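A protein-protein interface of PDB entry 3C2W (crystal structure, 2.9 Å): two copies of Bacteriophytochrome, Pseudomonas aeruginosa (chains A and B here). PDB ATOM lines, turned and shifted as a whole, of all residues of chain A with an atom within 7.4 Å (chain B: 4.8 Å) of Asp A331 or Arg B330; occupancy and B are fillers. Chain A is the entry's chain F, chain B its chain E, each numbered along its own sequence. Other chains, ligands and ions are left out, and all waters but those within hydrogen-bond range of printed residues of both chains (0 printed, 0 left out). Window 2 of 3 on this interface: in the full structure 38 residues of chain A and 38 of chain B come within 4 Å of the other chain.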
ATOM      1  N   LEU A 325      20.066   3.772   4.439  1.00  0.00           N
ATOM      2  CA  LEU A 325      20.389   3.194   3.140  1.00  0.00           C
ATOM      3  C   LEU A 325      19.536   1.967   2.848  1.00  0.00           C
ATOM      4  O   LEU A 325      19.226   1.681   1.689  1.00  0.00           O
ATOM      5  CB  LEU A 325      21.878   2.855   3.023  1.00  0.00           C
ATOM      6  CG  LEU A 325      22.555   1.927   4.033  1.00  0.00           C
ATOM      7  CD1 LEU A 325      22.002   0.506   3.994  1.00  0.00           C
ATOM      8  CD2 LEU A 325      24.045   1.902   3.753  1.00  0.00           C
ATOM      9  N   ALA A 326      19.155   1.243   3.895  1.00  0.00           N
ATOM     10  CA  ALA A 326      18.314   0.066   3.719  1.00  0.00           C
ATOM     11  C   ALA A 326      17.022   0.479   3.040  1.00  0.00           C
ATOM     12  O   ALA A 326      16.473  -0.252   2.222  1.00  0.00           O
ATOM     13  CB  ALA A 326      18.029  -0.593   5.054  1.00  0.00           C
ATOM     14  N   ARG A 327      16.556   1.672   3.386  1.00  0.00           N
ATOM     15  CA  ARG A 327      15.326   2.220   2.836  1.00  0.00           C
ATOM     16  C   ARG A 327      15.581   2.896   1.500  1.00  0.00           C
ATOM     17  O   ARG A 327      14.762   2.818   0.588  1.00  0.00           O
ATOM     18  CB  ARG A 327      14.720   3.241   3.802  1.00  0.00           C
ATOM     19  CG  ARG A 327      13.583   4.058   3.207  1.00  0.00           C
ATOM     20  CD  ARG A 327      13.324   5.329   3.997  1.00  0.00           C
ATOM     21  NE  ARG A 327      13.258   5.071   5.432  1.00  0.00           N
ATOM     22  CZ  ARG A 327      12.215   4.515   6.041  1.00  0.00           C
ATOM     23  NH1 ARG A 327      11.149   4.153   5.338  1.00  0.00           N
ATOM     24  NH2 ARG A 327      12.233   4.319   7.352  1.00  0.00           N
ATOM     25  N   ARG A 328      16.720   3.565   1.387  1.00  0.00           N
ATOM     26  CA  ARG A 328      17.027   4.323   0.183  1.00  0.00           C
ATOM     27  C   ARG A 328      17.312   3.401  -1.002  1.00  0.00           C
ATOM     28  O   ARG A 328      16.936   3.698  -2.137  1.00  0.00           O
ATOM     29  CB  ARG A 328      18.215   5.250   0.434  1.00  0.00           C
ATOM     30  CG  ARG A 328      18.319   6.401  -0.546  1.00  0.00           C
ATOM     31  CD  ARG A 328      19.229   7.495  -0.004  1.00  0.00           C
ATOM     32  NE  ARG A 328      18.830   7.957   1.328  1.00  0.00           N
ATOM     33  CZ  ARG A 328      19.454   7.629   2.458  1.00  0.00           C
ATOM     34  NH1 ARG A 328      20.516   6.831   2.425  1.00  0.00           N
ATOM     35  NH2 ARG A 328      19.016   8.102   3.620  1.00  0.00           N
ATOM     36  N   ALA A 329      17.969   2.276  -0.729  1.00  0.00           N
ATOM     37  CA  ALA A 329      18.365   1.340  -1.774  1.00  0.00           C
ATOM     38  C   ALA A 329      17.257   0.335  -2.094  1.00  0.00           C
ATOM     39  O   ALA A 329      17.295  -0.325  -3.131  1.00  0.00           O
ATOM     40  CB  ALA A 329      19.649   0.624  -1.382  1.00  0.00           C
ATOM     41  N   ARG A 330      16.283   0.213  -1.195  1.00  0.00           N
ATOM     42  CA  ARG A 330      15.181  -0.730  -1.379  1.00  0.00           C
ATOM     43  C   ARG A 330      13.947  -0.050  -1.965  1.00  0.00           C
ATOM     44  O   ARG A 330      13.036  -0.711  -2.469  1.00  0.00           O
ATOM     45  CB  ARG A 330      14.835  -1.421  -0.061  1.00  0.00           C
ATOM     46  CG  ARG A 330      13.648  -2.364  -0.149  1.00  0.00           C
ATOM     47  CD  ARG A 330      13.435  -3.139   1.145  1.00  0.00           C
ATOM     48  NE  ARG A 330      14.352  -4.270   1.276  1.00  0.00           N
ATOM     49  CZ  ARG A 330      15.354  -4.321   2.148  1.00  0.00           C
ATOM     50  NH1 ARG A 330      15.572  -3.299   2.966  1.00  0.00           N
ATOM     51  NH2 ARG A 330      16.138  -5.392   2.198  1.00  0.00           N
ATOM     52  N   ASP A 331      13.915   1.275  -1.893  1.00  0.00           N
ATOM     53  CA  ASP A 331      12.857   2.042  -2.544  1.00  0.00           C
ATOM     54  C   ASP A 331      13.373   2.535  -3.894  1.00  0.00           C
ATOM     55  O   ASP A 331      12.837   3.471  -4.489  1.00  0.00           O
ATOM     56  CB  ASP A 331      12.408   3.205  -1.661  1.00  0.00           C
ATOM     57  CG  ASP A 331      11.759   2.739  -0.367  1.00  0.00           C
ATOM     58  OD1 ASP A 331      11.502   3.585   0.511  1.00  0.00           O
ATOM     59  OD2 ASP A 331      11.502   1.523  -0.227  1.00  0.00           O
ATOM     60  N   ALA A 332      14.430   1.877  -4.358  1.00  0.00           N
ATOM     61  CA  ALA A 332      15.049   2.150  -5.643  1.00  0.00           C
ATOM     62  C   ALA A 332      15.950   0.961  -5.939  1.00  0.00           C
ATOM     63  O   ALA A 332      15.937  -0.029  -5.208  1.00  0.00           O
ATOM     64  CB  ALA A 332      15.846   3.432  -5.591  1.00  0.00           C
ATOM     65  N   ASP A 333      16.734   1.041  -7.004  1.00  0.00           N
ATOM     66  CA  ASP A 333      17.714  -0.005  -7.267  1.00  0.00           C
ATOM     67  C   ASP A 333      19.115   0.575  -7.207  1.00  0.00           C
ATOM     68  O   ASP A 333      20.070   0.008  -7.737  1.00  0.00           O
ATOM     69  CB  ASP A 333      17.436  -0.698  -8.603  1.00  0.00           C
ATOM     70  CG  ASP A 333      16.311  -1.711  -8.506  1.00  0.00           C
ATOM     71  OD1 ASP A 333      15.865  -1.993  -7.374  1.00  0.00           O
ATOM     72  OD2 ASP A 333      15.873  -2.223  -9.560  1.00  0.00           O
ATOM     73  N   ASP A 334      19.216   1.717  -6.536  1.00  0.00           N
ATOM     74  CA  ASP A 334      20.465   2.449  -6.433  1.00  0.00           C
ATOM     75  C   ASP A 334      21.208   2.075  -5.155  1.00  0.00           C
ATOM     76  O   ASP A 334      20.999   2.687  -4.103  1.00  0.00           O
ATOM     77  CB  ASP A 334      20.196   3.956  -6.454  1.00  0.00           C
ATOM     78  CG  ASP A 334      21.341   4.742  -7.056  1.00  0.00           C
ATOM     79  OD1 ASP A 334      22.233   4.109  -7.665  1.00  0.00           O
ATOM     80  OD2 ASP A 334      21.344   5.987  -6.923  1.00  0.00           O
ATOM     81  N   ASN A 495      18.733 -10.351  -2.349  1.00  0.00           N
ATOM     82  CA  ASN A 495      17.328  -9.961  -2.330  1.00  0.00           C
ATOM     83  C   ASN A 495      16.822  -9.494  -3.696  1.00  0.00           C
ATOM     84  O   ASN A 495      15.625  -9.286  -3.888  1.00  0.00           O
ATOM     85  CB  ASN A 495      17.080  -8.883  -1.271  1.00  0.00           C
ATOM     86  CG  ASN A 495      15.666  -8.923  -0.719  1.00  0.00           C
ATOM     87  OD1 ASN A 495      14.743  -9.407  -1.373  1.00  0.00           O
ATOM     88  ND2 ASN A 495      15.495  -8.426   0.500  1.00  0.00           N
ATOM     89  N   ALA B 326      11.521  -2.664   8.300  1.00  0.00           N
ATOM     90  CA  ALA B 326      11.820  -1.848   7.129  1.00  0.00           C
ATOM     91  C   ALA B 326      12.157  -2.770   5.958  1.00  0.00           C
ATOM     92  O   ALA B 326      11.949  -2.422   4.795  1.00  0.00           O
ATOM     93  CB  ALA B 326      12.971  -0.894   7.419  1.00  0.00           C
ATOM     94  N   ARG B 327      12.683  -3.949   6.279  1.00  0.00           N
ATOM     95  CA  ARG B 327      12.908  -4.987   5.283  1.00  0.00           C
ATOM     96  C   ARG B 327      11.606  -5.710   4.971  1.00  0.00           C
ATOM     97  O   ARG B 327      11.142  -5.720   3.833  1.00  0.00           O
ATOM     98  CB  ARG B 327      13.903  -6.022   5.798  1.00  0.00           C
ATOM     99  CG  ARG B 327      15.297  -5.511   6.084  1.00  0.00           C
ATOM    100  CD  ARG B 327      16.077  -6.625   6.746  1.00  0.00           C
ATOM    101  NE  ARG B 327      17.421  -6.235   7.150  1.00  0.00           N
ATOM    102  CZ  ARG B 327      18.051  -6.751   8.201  1.00  0.00           C
ATOM    103  NH1 ARG B 327      17.448  -7.668   8.947  1.00  0.00           N
ATOM    104  NH2 ARG B 327      19.279  -6.357   8.509  1.00  0.00           N
ATOM    105  N   ARG B 328      11.038  -6.336   5.996  1.00  0.00           N
ATOM    106  CA  ARG B 328       9.864  -7.183   5.840  1.00  0.00           C
ATOM    107  C   ARG B 328       8.719  -6.465   5.131  1.00  0.00           C
ATOM    108  O   ARG B 328       7.969  -7.073   4.368  1.00  0.00           O
ATOM    109  CB  ARG B 328       9.416  -7.708   7.206  1.00  0.00           C
ATOM    110  CG  ARG B 328      10.479  -8.537   7.909  1.00  0.00           C
ATOM    111  CD  ARG B 328      10.168  -8.755   9.377  1.00  0.00           C
ATOM    112  NE  ARG B 328      11.282  -9.389  10.079  1.00  0.00           N
ATOM    113  CZ  ARG B 328      11.358  -9.507  11.402  1.00  0.00           C
ATOM    114  NH1 ARG B 328      10.385  -9.028  12.170  1.00  0.00           N
ATOM    115  NH2 ARG B 328      12.405 -10.097  11.962  1.00  0.00           N
ATOM    116  N   ALA B 329       8.600  -5.165   5.375  1.00  0.00           N
ATOM    117  CA  ALA B 329       7.455  -4.395   4.891  1.00  0.00           C
ATOM    118  C   ALA B 329       7.575  -3.948   3.433  1.00  0.00           C
ATOM    119  O   ALA B 329       6.575  -3.858   2.726  1.00  0.00           O
ATOM    120  CB  ALA B 329       7.204  -3.199   5.791  1.00  0.00           C
ATOM    121  N   ARG B 330       8.793  -3.660   2.986  1.00  0.00           N
ATOM    122  CA  ARG B 330       9.007  -3.320   1.583  1.00  0.00           C
ATOM    123  C   ARG B 330       9.265  -4.561   0.735  1.00  0.00           C
ATOM    124  O   ARG B 330       9.146  -4.514  -0.486  1.00  0.00           O
ATOM    125  CB  ARG B 330      10.134  -2.291   1.424  1.00  0.00           C
ATOM    126  CG  ARG B 330       9.675  -0.842   1.583  1.00  0.00           C
ATOM    127  CD  ARG B 330       9.167  -0.262   0.266  1.00  0.00           C
ATOM    128  NE  ARG B 330       8.008   0.603   0.461  1.00  0.00           N
ATOM    129  CZ  ARG B 330       6.842   0.430  -0.153  1.00  0.00           C
ATOM    130  NH1 ARG B 330       6.692  -0.556  -1.021  1.00  0.00           N
ATOM    131  NH2 ARG B 330       5.828   1.253   0.081  1.00  0.00           N
ATOM    132  N   ASP B 331       9.599  -5.669   1.392  1.00  0.00           N
ATOM    133  CA  ASP B 331       9.850  -6.935   0.704  1.00  0.00           C
ATOM    134  C   ASP B 331       8.569  -7.567   0.139  1.00  0.00           C
ATOM    135  O   ASP B 331       8.604  -8.198  -0.916  1.00  0.00           O
ATOM    136  CB  ASP B 331      10.562  -7.924   1.637  1.00  0.00           C
ATOM    137  CG  ASP B 331      12.023  -7.567   1.865  1.00  0.00           C
ATOM    138  OD1 ASP B 331      12.480  -6.540   1.320  1.00  0.00           O
ATOM    139  OD2 ASP B 331      12.708  -8.316   2.591  1.00  0.00           O
ATOM    140  N   ALA B 332       7.444  -7.404   0.833  1.00  0.00           N
ATOM    141  CA  ALA B 332       6.183  -8.021   0.408  1.00  0.00           C
ATOM    142  C   ALA B 332       5.131  -6.976   0.030  1.00  0.00           C
ATOM    143  O   ALA B 332       4.317  -7.200  -0.864  1.00  0.00           O
ATOM    144  CB  ALA B 332       5.658  -8.951   1.487  1.00  0.00           C
ATOM    145  N   ASP B 333       5.134  -5.864   0.759  1.00  0.00           N
ATOM    146  CA  ASP B 333       4.470  -4.609   0.359  1.00  0.00           C
ATOM    147  C   ASP B 333       3.129  -4.223   1.009  1.00  0.00           C
ATOM    148  O   ASP B 333       2.624  -3.128   0.761  1.00  0.00           O
ATOM    149  CB  ASP B 333       4.406  -4.441  -1.169  1.00  0.00           C
ATOM    150  CG  ASP B 333       4.748  -3.029  -1.600  1.00  0.00           C
ATOM    151  OD1 ASP B 333       4.987  -2.196  -0.700  1.00  0.00           O
ATOM    152  OD2 ASP B 333       4.790  -2.762  -2.821  1.00  0.00           O
ATOM    153  N   LEU B 492       7.021   5.177   4.748  1.00  0.00           N
ATOM    154  CA  LEU B 492       6.816   3.832   4.229  1.00  0.00           C
ATOM    155  C   LEU B 492       5.453   3.712   3.566  1.00  0.00           C
ATOM    156  O   LEU B 492       5.311   3.039   2.554  1.00  0.00           O
ATOM    157  CB  LEU B 492       6.941   2.796   5.341  1.00  0.00           C
ATOM    158  CG  LEU B 492       7.234   1.376   4.865  1.00  0.00           C
ATOM    159  CD1 LEU B 492       8.706   1.249   4.498  1.00  0.00           C
ATOM    160  CD2 LEU B 492       6.855   0.373   5.939  1.00  0.00           C
ATOM    161  N   ASN B 495       5.091   6.066  -0.050  1.00  0.00           N
ATOM    162  CA  ASN B 495       5.726   5.519  -1.248  1.00  0.00           C
ATOM    163  C   ASN B 495       5.764   3.992  -1.280  1.00  0.00           C
ATOM    164  O   ASN B 495       4.774   3.320  -1.571  1.00  0.00           O
ATOM    165  CB  ASN B 495       7.153   6.064  -1.381  1.00  0.00           C
ATOM    166  CG  ASN B 495       7.184   7.547  -1.681  1.00  0.00           C
ATOM    167  OD1 ASN B 495       7.007   7.959  -2.827  1.00  0.00           O
ATOM    168  ND2 ASN B 495       7.417   8.360  -0.653  1.00  0.00           N
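Printed residues of chain B that touch a printed residue of chain A: Arg B327, Arg B330, Asp B331 and Leu B492. Along chain B the printed residues that touch a printed residue of chain A span positions 327 to 492. Among the printed residues, 6 pairs touch across the chains. Among the printed residues, Asp or Glu carboxylates within 4 Å of a Lys or Arg side-chain nitrogen of the other chain: Arg A330 with Asp B331 and Asp A331 with Arg B330.
NH2 of Arg B330 lies within hydrogen-bond range of O of Asn B495 (2.8 Å). The guanidinium group of Arg A330 lies close to the backbone carbonyl oxygen of Ala A326 (3.3 Å). The guanidinium group (NH1) of Arg B330 is in salt-bridge range of the side-chain carboxylate (OD2) of Asp B333 (3.4 Å). The guanidinium group (NH2) of Arg B330 lies within hydrogen-bond range of the backbone carbonyl oxygen (O) of Leu B492 (3.1 Å).
Printed residues of chain B within 4 Å of Arg A330: Arg B327 (3.8 Å), Arg B330 (3.4 Å) and Asp B331 (2.9 Å). Of chain B, only Arg B330 (3.0 Å) comes within 4 Å of Asp A331. Printed residues of chain B within 4 Å of Asn A495: Asp B331. Of the printed residues of chain A, Arg B327 touches Arg A330 (3.8 Å). No residue of chain A comes within 4 Å of Ala B329. Of the printed residues of chain A, Asp B331 touches Arg A330 (2.9 Å) and Asn A495 (3.5 Å). The nearest printed residue of chain B that does not touch Asp A331 is Asn B495 (5.4 Å). The nearest printed residue of chain A that does not touch Arg B327 is Ala A326 (5.7 Å).
Arg A330 touches Arg B327, but with the chains exchanged Arg A327 does not touch Arg B330 (6.3 Å). Arg B330 touches its own counterpart, Arg A330. Arg A330 touches Asp B331, and with the chains exchanged Asp A331 touches Arg B330. Asn A495 touches Asp B331, but with the chains exchanged Asp A331 does not touch Asn B495 (5.4 Å). 9 positions are printed for both chains. Of the 6 pairs that touch across the chains among the printed residues, 3 have their exchanged pair printed and touching as well.
The side-chain carboxylate of Asp A331 lies within salt-bridge range of the guanidinium group of Arg B330, at 3.7 Å. OD1 of Asp B331 lies within salt-bridge range of NE of Arg A330, at 2.9 Å. The side-chain carboxylate of Asp B331 sits at hydrogen-bond distance from the side-chain amide nitrogen of Asn A495, at 3.5 Å.
Among the printed residues, pairs that only touch across the chains: Arg A330 with Arg B330 (3.4 Å), Arg A330 with Arg B327 (3.8 Å) and Arg A327 with Leu B492 (3.9 Å).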
